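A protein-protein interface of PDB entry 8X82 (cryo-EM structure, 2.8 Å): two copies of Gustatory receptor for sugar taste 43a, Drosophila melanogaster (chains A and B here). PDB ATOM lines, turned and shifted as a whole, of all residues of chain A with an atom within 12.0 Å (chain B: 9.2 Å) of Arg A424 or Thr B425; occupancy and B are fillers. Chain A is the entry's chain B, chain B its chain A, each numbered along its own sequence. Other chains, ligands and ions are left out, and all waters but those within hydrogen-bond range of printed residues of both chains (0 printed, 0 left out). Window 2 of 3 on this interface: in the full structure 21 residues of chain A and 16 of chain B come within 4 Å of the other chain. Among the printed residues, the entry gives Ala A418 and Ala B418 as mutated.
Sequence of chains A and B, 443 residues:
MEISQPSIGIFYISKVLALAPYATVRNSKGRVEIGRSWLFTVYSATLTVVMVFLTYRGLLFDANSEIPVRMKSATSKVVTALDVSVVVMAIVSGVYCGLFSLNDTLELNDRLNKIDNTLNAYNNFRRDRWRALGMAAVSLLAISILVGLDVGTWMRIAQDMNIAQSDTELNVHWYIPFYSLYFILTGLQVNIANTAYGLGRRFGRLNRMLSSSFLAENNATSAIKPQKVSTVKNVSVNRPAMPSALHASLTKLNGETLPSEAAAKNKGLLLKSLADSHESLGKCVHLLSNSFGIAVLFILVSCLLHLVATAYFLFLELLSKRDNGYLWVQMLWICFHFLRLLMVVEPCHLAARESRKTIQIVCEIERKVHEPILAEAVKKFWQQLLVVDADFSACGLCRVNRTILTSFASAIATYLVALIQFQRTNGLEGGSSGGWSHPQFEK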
ATOM      1  N   THR A  75      39.846 -26.753  -0.840  1.00  0.00           N
ATOM      2  CA  THR A  75      38.424 -26.781  -1.165  1.00  0.00           C
ATOM      3  C   THR A  75      38.175 -26.203  -2.552  1.00  0.00           C
ATOM      4  O   THR A  75      37.411 -26.765  -3.347  1.00  0.00           O
ATOM      5  CB  THR A  75      37.630 -26.013  -0.105  1.00  0.00           C
ATOM      6  OG1 THR A  75      37.561 -26.790   1.097  1.00  0.00           O
ATOM      7  CG2 THR A  75      36.219 -25.720  -0.593  1.00  0.00           C
ATOM      8  N   TYR A 312      27.250 -23.166  -3.410  1.00  0.00           N
ATOM      9  CA  TYR A 312      28.182 -23.140  -2.287  1.00  0.00           C
ATOM     10  C   TYR A 312      29.180 -21.994  -2.424  1.00  0.00           C
ATOM     11  O   TYR A 312      29.474 -21.297  -1.445  1.00  0.00           O
ATOM     12  CB  TYR A 312      28.905 -24.483  -2.182  1.00  0.00           C
ATOM     13  CG  TYR A 312      29.989 -24.532  -1.133  1.00  0.00           C
ATOM     14  CD1 TYR A 312      29.672 -24.576   0.218  1.00  0.00           C
ATOM     15  CD2 TYR A 312      31.331 -24.553  -1.491  1.00  0.00           C
ATOM     16  CE1 TYR A 312      30.659 -24.626   1.183  1.00  0.00           C
ATOM     17  CE2 TYR A 312      32.326 -24.605  -0.531  1.00  0.00           C
ATOM     18  CZ  TYR A 312      31.983 -24.641   0.804  1.00  0.00           C
ATOM     19  OH  TYR A 312      32.969 -24.693   1.762  1.00  0.00           O
ATOM     20  N   PHE A 315      27.409 -18.800  -1.625  1.00  0.00           N
ATOM     21  CA  PHE A 315      27.302 -18.618  -0.182  1.00  0.00           C
ATOM     22  C   PHE A 315      28.625 -18.147   0.408  1.00  0.00           C
ATOM     23  O   PHE A 315      28.646 -17.291   1.299  1.00  0.00           O
ATOM     24  CB  PHE A 315      26.825 -19.918   0.478  1.00  0.00           C
ATOM     25  CG  PHE A 315      27.295 -20.103   1.903  1.00  0.00           C
ATOM     26  CD1 PHE A 315      28.554 -20.619   2.187  1.00  0.00           C
ATOM     27  CD2 PHE A 315      26.471 -19.757   2.962  1.00  0.00           C
ATOM     28  CE1 PHE A 315      28.976 -20.781   3.492  1.00  0.00           C
ATOM     29  CE2 PHE A 315      26.889 -19.919   4.269  1.00  0.00           C
ATOM     30  CZ  PHE A 315      28.143 -20.433   4.534  1.00  0.00           C
ATOM     31  N   LEU A 316      29.743 -18.709  -0.064  1.00  0.00           N
ATOM     32  CA  LEU A 316      31.048 -18.289   0.436  1.00  0.00           C
ATOM     33  C   LEU A 316      31.316 -16.823   0.119  1.00  0.00           C
ATOM     34  O   LEU A 316      31.784 -16.069   0.981  1.00  0.00           O
ATOM     35  CB  LEU A 316      32.150 -19.167  -0.153  1.00  0.00           C
ATOM     36  CG  LEU A 316      32.206 -20.630   0.288  1.00  0.00           C
ATOM     37  CD1 LEU A 316      33.475 -21.283  -0.233  1.00  0.00           C
ATOM     38  CD2 LEU A 316      32.132 -20.734   1.800  1.00  0.00           C
ATOM     39  N   LEU A 319      29.103 -14.642   2.265  1.00  0.00           N
ATOM     40  CA  LEU A 319      29.637 -14.550   3.619  1.00  0.00           C
ATOM     41  C   LEU A 319      30.840 -13.616   3.672  1.00  0.00           C
ATOM     42  O   LEU A 319      30.986 -12.825   4.611  1.00  0.00           O
ATOM     43  CB  LEU A 319      30.011 -15.944   4.125  1.00  0.00           C
ATOM     44  CG  LEU A 319      30.180 -16.118   5.634  1.00  0.00           C
ATOM     45  CD1 LEU A 319      28.854 -16.494   6.276  1.00  0.00           C
ATOM     46  CD2 LEU A 319      31.238 -17.167   5.933  1.00  0.00           C
ATOM     47  N   SER A 320      31.717 -13.697   2.668  1.00  0.00           N
ATOM     48  CA  SER A 320      32.907 -12.852   2.654  1.00  0.00           C
ATOM     49  C   SER A 320      32.574 -11.421   2.245  1.00  0.00           C
ATOM     50  O   SER A 320      33.188 -10.472   2.745  1.00  0.00           O
ATOM     51  CB  SER A 320      33.959 -13.446   1.719  1.00  0.00           C
ATOM     52  OG  SER A 320      35.020 -12.533   1.499  1.00  0.00           O
ATOM     53  N   TYR A 415      23.032 -31.622   0.430  1.00  0.00           N
ATOM     54  CA  TYR A 415      24.471 -31.453   0.249  1.00  0.00           C
ATOM     55  C   TYR A 415      24.908 -30.029   0.570  1.00  0.00           C
ATOM     56  O   TYR A 415      25.991 -29.822   1.128  1.00  0.00           O
ATOM     57  CB  TYR A 415      24.880 -31.831  -1.175  1.00  0.00           C
ATOM     58  CG  TYR A 415      24.593 -33.271  -1.532  1.00  0.00           C
ATOM     59  CD1 TYR A 415      24.892 -34.298  -0.649  1.00  0.00           C
ATOM     60  CD2 TYR A 415      24.042 -33.606  -2.761  1.00  0.00           C
ATOM     61  CE1 TYR A 415      24.634 -35.615  -0.971  1.00  0.00           C
ATOM     62  CE2 TYR A 415      23.782 -34.919  -3.094  1.00  0.00           C
ATOM     63  CZ  TYR A 415      24.080 -35.919  -2.196  1.00  0.00           C
ATOM     64  OH  TYR A 415      23.822 -37.230  -2.524  1.00  0.00           O
ATOM     65  N   LEU A 416      24.085 -29.036   0.225  1.00  0.00           N
ATOM     66  CA  LEU A 416      24.441 -27.653   0.520  1.00  0.00           C
ATOM     67  C   LEU A 416      24.543 -27.418   2.020  1.00  0.00           C
ATOM     68  O   LEU A 416      25.520 -26.828   2.496  1.00  0.00           O
ATOM     69  CB  LEU A 416      23.420 -26.700  -0.100  1.00  0.00           C
ATOM     70  CG  LEU A 416      23.940 -25.349  -0.588  1.00  0.00           C
ATOM     71  CD1 LEU A 416      25.305 -25.500  -1.241  1.00  0.00           C
ATOM     72  CD2 LEU A 416      22.946 -24.719  -1.548  1.00  0.00           C
ATOM     73  N   VAL A 417      23.551 -27.884   2.783  1.00  0.00           N
ATOM     74  CA  VAL A 417      23.581 -27.695   4.231  1.00  0.00           C
ATOM     75  C   VAL A 417      24.780 -28.415   4.836  1.00  0.00           C
ATOM     76  O   VAL A 417      25.460 -27.888   5.727  1.00  0.00           O
ATOM     77  CB  VAL A 417      22.256 -28.169   4.856  1.00  0.00           C
ATOM     78  CG1 VAL A 417      22.404 -28.331   6.354  1.00  0.00           C
ATOM     79  CG2 VAL A 417      21.139 -27.192   4.532  1.00  0.00           C
ATOM     80  N   ALA A 418      25.066 -29.626   4.351  1.00  0.00           N
ATOM     81  CA  ALA A 418      26.237 -30.352   4.829  1.00  0.00           C
ATOM     82  C   ALA A 418      27.522 -29.588   4.525  1.00  0.00           C
ATOM     83  O   ALA A 418      28.450 -29.571   5.341  1.00  0.00           O
ATOM     84  CB  ALA A 418      26.276 -31.746   4.206  1.00  0.00           C
ATOM     85  N   LEU A 419      27.595 -28.950   3.355  1.00  0.00           N
ATOM     86  CA  LEU A 419      28.780 -28.167   3.016  1.00  0.00           C
ATOM     87  C   LEU A 419      28.903 -26.930   3.899  1.00  0.00           C
ATOM     88  O   LEU A 419      30.017 -26.489   4.206  1.00  0.00           O
ATOM     89  CB  LEU A 419      28.752 -27.776   1.540  1.00  0.00           C
ATOM     90  CG  LEU A 419      28.987 -28.904   0.534  1.00  0.00           C
ATOM     91  CD1 LEU A 419      29.152 -28.345  -0.869  1.00  0.00           C
ATOM     92  CD2 LEU A 419      30.196 -29.734   0.932  1.00  0.00           C
ATOM     93  N   ILE A 420      27.775 -26.344   4.302  1.00  0.00           N
ATOM     94  CA  ILE A 420      27.827 -25.210   5.224  1.00  0.00           C
ATOM     95  C   ILE A 420      28.424 -25.644   6.556  1.00  0.00           C
ATOM     96  O   ILE A 420      29.281 -24.959   7.129  1.00  0.00           O
ATOM     97  CB  ILE A 420      26.430 -24.588   5.411  1.00  0.00           C
ATOM     98  CG1 ILE A 420      25.789 -24.258   4.064  1.00  0.00           C
ATOM     99  CG2 ILE A 420      26.523 -23.333   6.254  1.00  0.00           C
ATOM    100  CD1 ILE A 420      26.656 -23.430   3.153  1.00  0.00           C
ATOM    101  N   GLN A 421      27.981 -26.796   7.067  1.00  0.00           N
ATOM    102  CA  GLN A 421      28.564 -27.330   8.294  1.00  0.00           C
ATOM    103  C   GLN A 421      30.038 -27.667   8.099  1.00  0.00           C
ATOM    104  O   GLN A 421      30.841 -27.542   9.031  1.00  0.00           O
ATOM    105  CB  GLN A 421      27.787 -28.561   8.754  1.00  0.00           C
ATOM    106  CG  GLN A 421      26.513 -28.239   9.510  1.00  0.00           C
ATOM    107  CD  GLN A 421      25.395 -29.216   9.211  1.00  0.00           C
ATOM    108  OE1 GLN A 421      25.641 -30.370   8.859  1.00  0.00           O
ATOM    109  NE2 GLN A 421      24.158 -28.757   9.344  1.00  0.00           N
ATOM    110  N   PHE A 422      30.406 -28.105   6.893  1.00  0.00           N
ATOM    111  CA  PHE A 422      31.812 -28.337   6.578  1.00  0.00           C
ATOM    112  C   PHE A 422      32.623 -27.051   6.686  1.00  0.00           C
ATOM    113  O   PHE A 422      33.726 -27.049   7.244  1.00  0.00           O
ATOM    114  CB  PHE A 422      31.933 -28.930   5.174  1.00  0.00           C
ATOM    115  CG  PHE A 422      33.345 -29.229   4.755  1.00  0.00           C
ATOM    116  CD1 PHE A 422      33.930 -30.447   5.052  1.00  0.00           C
ATOM    117  CD2 PHE A 422      34.083 -28.294   4.047  1.00  0.00           C
ATOM    118  CE1 PHE A 422      35.226 -30.722   4.657  1.00  0.00           C
ATOM    119  CE2 PHE A 422      35.380 -28.561   3.656  1.00  0.00           C
ATOM    120  CZ  PHE A 422      35.952 -29.778   3.961  1.00  0.00           C
ATOM    121  N   GLN A 423      32.093 -25.949   6.152  1.00  0.00           N
ATOM    122  CA  GLN A 423      32.849 -24.701   6.134  1.00  0.00           C
ATOM    123  C   GLN A 423      32.988 -24.112   7.532  1.00  0.00           C
ATOM    124  O   GLN A 423      34.053 -23.595   7.890  1.00  0.00           O
ATOM    125  CB  GLN A 423      32.185 -23.695   5.192  1.00  0.00           C
ATOM    126  CG  GLN A 423      32.912 -22.357   5.088  1.00  0.00           C
ATOM    127  CD  GLN A 423      34.193 -22.424   4.269  1.00  0.00           C
ATOM    128  OE1 GLN A 423      34.932 -21.444   4.180  1.00  0.00           O
ATOM    129  NE2 GLN A 423      34.449 -23.572   3.649  1.00  0.00           N
ATOM    130  N   ARG A 424      31.922 -24.172   8.336  1.00  0.00           N
ATOM    131  CA  ARG A 424      31.989 -23.598   9.677  1.00  0.00           C
ATOM    132  C   ARG A 424      32.989 -24.342  10.553  1.00  0.00           C
ATOM    133  O   ARG A 424      33.725 -23.722  11.330  1.00  0.00           O
ATOM    134  CB  ARG A 424      30.606 -23.596  10.323  1.00  0.00           C
ATOM    135  CG  ARG A 424      29.699 -22.487   9.832  1.00  0.00           C
ATOM    136  CD  ARG A 424      28.454 -22.387  10.689  1.00  0.00           C
ATOM    137  NE  ARG A 424      28.769 -22.272  12.108  1.00  0.00           N
ATOM    138  CZ  ARG A 424      28.868 -21.123  12.763  1.00  0.00           C
ATOM    139  NH1 ARG A 424      28.682 -19.963  12.155  1.00  0.00           N
ATOM    140  NH2 ARG A 424      29.161 -21.139  14.061  1.00  0.00           N
ATOM    141  N   THR A 425      33.027 -25.667  10.450  1.00  0.00           N
ATOM    142  CA  THR A 425      33.938 -26.475  11.254  1.00  0.00           C
ATOM    143  C   THR A 425      35.395 -26.187  10.903  1.00  0.00           C
ATOM    144  O   THR A 425      35.696 -25.670   9.828  1.00  0.00           O
ATOM    145  CB  THR A 425      33.666 -27.979  11.071  1.00  0.00           C
ATOM    146  OG1 THR A 425      32.412 -28.318  11.676  1.00  0.00           O
ATOM    147  CG2 THR A 425      34.770 -28.801  11.714  1.00  0.00           C
ATOM    148  N   ALA B  74      22.290 -12.644  11.457  1.00  0.00           N
ATOM    149  CA  ALA B  74      22.386 -13.154  10.093  1.00  0.00           C
ATOM    150  C   ALA B  74      21.526 -14.399   9.911  1.00  0.00           C
ATOM    151  O   ALA B  74      20.826 -14.536   8.901  1.00  0.00           O
ATOM    152  CB  ALA B  74      23.843 -13.451   9.742  1.00  0.00           C
ATOM    153  N   THR B  75      21.564 -15.315  10.880  1.00  0.00           N
ATOM    154  CA  THR B  75      20.667 -16.465  10.846  1.00  0.00           C
ATOM    155  C   THR B  75      19.213 -16.017  10.927  1.00  0.00           C
ATOM    156  O   THR B  75      18.354 -16.507  10.184  1.00  0.00           O
ATOM    157  CB  THR B  75      21.005 -17.427  11.986  1.00  0.00           C
ATOM    158  OG1 THR B  75      22.216 -18.130  11.677  1.00  0.00           O
ATOM    159  CG2 THR B  75      19.883 -18.435  12.195  1.00  0.00           C
ATOM    160  N   TYR B 312      12.801 -24.795  14.268  1.00  0.00           N
ATOM    161  CA  TYR B 312      14.164 -24.399  14.611  1.00  0.00           C
ATOM    162  C   TYR B 312      14.169 -23.209  15.565  1.00  0.00           C
ATOM    163  O   TYR B 312      14.939 -23.182  16.532  1.00  0.00           O
ATOM    164  CB  TYR B 312      14.947 -24.081  13.336  1.00  0.00           C
ATOM    165  CG  TYR B 312      16.335 -23.536  13.572  1.00  0.00           C
ATOM    166  CD1 TYR B 312      17.358 -24.361  14.020  1.00  0.00           C
ATOM    167  CD2 TYR B 312      16.630 -22.201  13.334  1.00  0.00           C
ATOM    168  CE1 TYR B 312      18.632 -23.871  14.233  1.00  0.00           C
ATOM    169  CE2 TYR B 312      17.902 -21.701  13.542  1.00  0.00           C
ATOM    170  CZ  TYR B 312      18.898 -22.540  13.992  1.00  0.00           C
ATOM    171  OH  TYR B 312      20.165 -22.047  14.202  1.00  0.00           O
ATOM    172  N   VAL B 417      17.759 -31.551  12.247  1.00  0.00           N
ATOM    173  CA  VAL B 417      18.954 -32.054  12.919  1.00  0.00           C
ATOM    174  C   VAL B 417      20.201 -31.375  12.366  1.00  0.00           C
ATOM    175  O   VAL B 417      21.114 -31.005  13.117  1.00  0.00           O
ATOM    176  CB  VAL B 417      19.033 -33.586  12.787  1.00  0.00           C
ATOM    177  CG1 VAL B 417      20.419 -34.078  13.140  1.00  0.00           C
ATOM    178  CG2 VAL B 417      17.989 -34.248  13.670  1.00  0.00           C
ATOM    179  N   ALA B 418      20.252 -31.188  11.045  1.00  0.00           N
ATOM    180  CA  ALA B 418      21.379 -30.483  10.445  1.00  0.00           C
ATOM    181  C   ALA B 418      21.475 -29.052  10.962  1.00  0.00           C
ATOM    182  O   ALA B 418      22.578 -28.541  11.192  1.00  0.00           O
ATOM    183  CB  ALA B 418      21.254 -30.502   8.924  1.00  0.00           C
ATOM    184  N   LEU B 419      20.333 -28.389  11.153  1.00  0.00           N
ATOM    185  CA  LEU B 419      20.350 -27.028  11.684  1.00  0.00           C
ATOM    186  C   LEU B 419      20.812 -27.002  13.136  1.00  0.00           C
ATOM    187  O   LEU B 419      21.444 -26.033  13.574  1.00  0.00           O
ATOM    188  CB  LEU B 419      18.970 -26.389  11.544  1.00  0.00           C
ATOM    189  CG  LEU B 419      18.531 -26.024  10.126  1.00  0.00           C
ATOM    190  CD1 LEU B 419      17.253 -25.203  10.154  1.00  0.00           C
ATOM    191  CD2 LEU B 419      19.636 -25.277   9.398  1.00  0.00           C
ATOM    192  N   ILE B 420      20.493 -28.045  13.906  1.00  0.00           N
ATOM    193  CA  ILE B 420      20.985 -28.119  15.280  1.00  0.00           C
ATOM    194  C   ILE B 420      22.507 -28.203  15.288  1.00  0.00           C
ATOM    195  O   ILE B 420      23.184 -27.516  16.065  1.00  0.00           O
ATOM    196  CB  ILE B 420      20.355 -29.308  16.027  1.00  0.00           C
ATOM    197  CG1 ILE B 420      18.830 -29.280  15.921  1.00  0.00           C
ATOM    198  CG2 ILE B 420      20.763 -29.289  17.487  1.00  0.00           C
ATOM    199  CD1 ILE B 420      18.207 -27.969  16.320  1.00  0.00           C
ATOM    200  N   GLN B 421      23.067 -29.047  14.418  1.00  0.00           N
ATOM    201  CA  GLN B 421      24.521 -29.123  14.297  1.00  0.00           C
ATOM    202  C   GLN B 421      25.100 -27.800  13.808  1.00  0.00           C
ATOM    203  O   GLN B 421      26.215 -27.424  14.187  1.00  0.00           O
ATOM    204  CB  GLN B 421      24.912 -30.262  13.359  1.00  0.00           C
ATOM    205  CG  GLN B 421      24.903 -31.631  14.013  1.00  0.00           C
ATOM    206  CD  GLN B 421      24.425 -32.720  13.076  1.00  0.00           C
ATOM    207  OE1 GLN B 421      24.556 -32.608  11.856  1.00  0.00           O
ATOM    208  NE2 GLN B 421      23.862 -33.781  13.641  1.00  0.00           N
ATOM    209  N   PHE B 422      24.357 -27.091  12.957  1.00  0.00           N
ATOM    210  CA  PHE B 422      24.774 -25.759  12.530  1.00  0.00           C
ATOM    211  C   PHE B 422      24.868 -24.802  13.711  1.00  0.00           C
ATOM    212  O   PHE B 422      25.830 -24.035  13.825  1.00  0.00           O
ATOM    213  CB  PHE B 422      23.797 -25.224  11.482  1.00  0.00           C
ATOM    214  CG  PHE B 422      24.147 -23.861  10.957  1.00  0.00           C
ATOM    215  CD1 PHE B 422      24.999 -23.716   9.876  1.00  0.00           C
ATOM    216  CD2 PHE B 422      23.611 -22.723  11.536  1.00  0.00           C
ATOM    217  CE1 PHE B 422      25.312 -22.460   9.389  1.00  0.00           C
ATOM    218  CE2 PHE B 422      23.925 -21.466  11.056  1.00  0.00           C
ATOM    219  CZ  PHE B 422      24.778 -21.335   9.981  1.00  0.00           C
ATOM    220  N   GLN B 423      23.870 -24.829  14.598  1.00  0.00           N
ATOM    221  CA  GLN B 423      23.842 -23.880  15.707  1.00  0.00           C
ATOM    222  C   GLN B 423      24.930 -24.180  16.728  1.00  0.00           C
ATOM    223  O   GLN B 423      25.563 -23.259  17.258  1.00  0.00           O
ATOM    224  CB  GLN B 423      22.465 -23.887  16.371  1.00  0.00           C
ATOM    225  CG  GLN B 423      22.324 -22.910  17.536  1.00  0.00           C
ATOM    226  CD  GLN B 423      22.212 -21.457  17.099  1.00  0.00           C
ATOM    227  OE1 GLN B 423      22.190 -20.551  17.933  1.00  0.00           O
ATOM    228  NE2 GLN B 423      22.116 -21.229  15.793  1.00  0.00           N
ATOM    229  N   ARG B 424      25.161 -25.462  17.026  1.00  0.00           N
ATOM    230  CA  ARG B 424      26.174 -25.808  18.018  1.00  0.00           C
ATOM    231  C   ARG B 424      27.571 -25.420  17.552  1.00  0.00           C
ATOM    232  O   ARG B 424      28.386 -24.935  18.346  1.00  0.00           O
ATOM    233  CB  ARG B 424      26.113 -27.299  18.342  1.00  0.00           C
ATOM    234  CG  ARG B 424      24.984 -27.679  19.278  1.00  0.00           C
ATOM    235  CD  ARG B 424      25.134 -29.108  19.757  1.00  0.00           C
ATOM    236  NE  ARG B 424      26.452 -29.362  20.328  1.00  0.00           N
ATOM    237  CZ  ARG B 424      26.733 -29.285  21.622  1.00  0.00           C
ATOM    238  NH1 ARG B 424      25.809 -28.964  22.512  1.00  0.00           N
ATOM    239  NH2 ARG B 424      27.973 -29.538  22.032  1.00  0.00           N
ATOM    240  N   THR B 425      27.868 -25.628  16.273  1.00  0.00           N
ATOM    241  CA  THR B 425      29.182 -25.303  15.727  1.00  0.00           C
ATOM    242  C   THR B 425      29.447 -23.800  15.769  1.00  0.00           C
ATOM    243  O   THR B 425      28.519 -22.997  15.863  1.00  0.00           O
ATOM    244  CB  THR B 425      29.326 -25.796  14.275  1.00  0.00           C
ATOM    245  OG1 THR B 425      29.380 -27.229  14.256  1.00  0.00           O
ATOM    246  CG2 THR B 425      30.591 -25.238  13.646  1.00  0.00           C
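O of Ala B418 lies within hydrogen-bond range of NE2 of Gln A421 (2.4 Å).
The backbone carbonyl oxygen of Thr B425 sits at hydrogen-bond distance from the guanidinium group of Arg A424 (2.7 Å).
The backbone carbonyl oxygen (O) of Gln B421 is in hydrogen-bond range of the side-chain hydroxyl (OG1) of Thr B425 (3.2 Å).
The backbone carbonyl oxygen of Gln A421 lies within hydrogen-bond range of the side-chain hydroxyl of Thr A425, 3.2 Å away.
Ala B418 touches Val A417.
CE1 of Phe B422 touches CG2 of Ile A420 (3.5 Å).
Gln A421 touches Gln B421 (OE1 to OE1, 3.9 Å).
Gln A421 touches Phe B422 (NE2 to N, 3.98 Å).
Arg A424 touches Phe B422.
Of the printed residues of chain B, Val A417 touches Ala B418.
Printed residues of chain B within 4 Å of Ile A420: Phe B422.
Of chain B, only Phe B422 (3.4 Å) and Thr B425 (2.7 Å) come within 4 Å of Arg A424.
Thr A425 touches none of the printed residues of chain B.
Printed residues of chain A within 4 Å of Ala B418: Val A417 and Gln A421.
Of the printed residues of chain A, Gln B421 touches Gln A421.
No residue of chain A comes within 4 Å of Gln B423.
The nearest residue of chain B that does not touch Arg A424 is Gln B423 (5.3 Å).
The nearest printed residue of chain B that does not touch Gln A421 is Leu B419 (4.2 Å).
Of the 17 printed residues of chain A, 4 touch a printed residue of chain B.
Printed residues of chain A that touch a printed residue of chain B: Val A417, Ile A420, Gln A421 and Arg A424.
Among the printed residues, 7 pairs touch across the chains.
Among the printed residues, no Asp or Glu carboxylate lies within 4 Å of a Lys or Arg side-chain nitrogen of the other chain.
Ile A420 touches Phe B422, but with the chains exchanged Phe A422 does not touch Ile B420 (11.5 Å).
Gln A421 touches Ala B418, but with the chains exchanged Ala A418 does not touch Gln B421 (7.6 Å).
Gln B421 touches its own counterpart, Gln A421.
Gln A421 touches Phe B422, but with the chains exchanged Phe A422 does not touch Gln B421 (8.4 Å).
11 positions are printed for both chains.
Of the 7 pairs that touch across the chains among the printed residues, 1 has its exchanged pair printed and touching as well.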
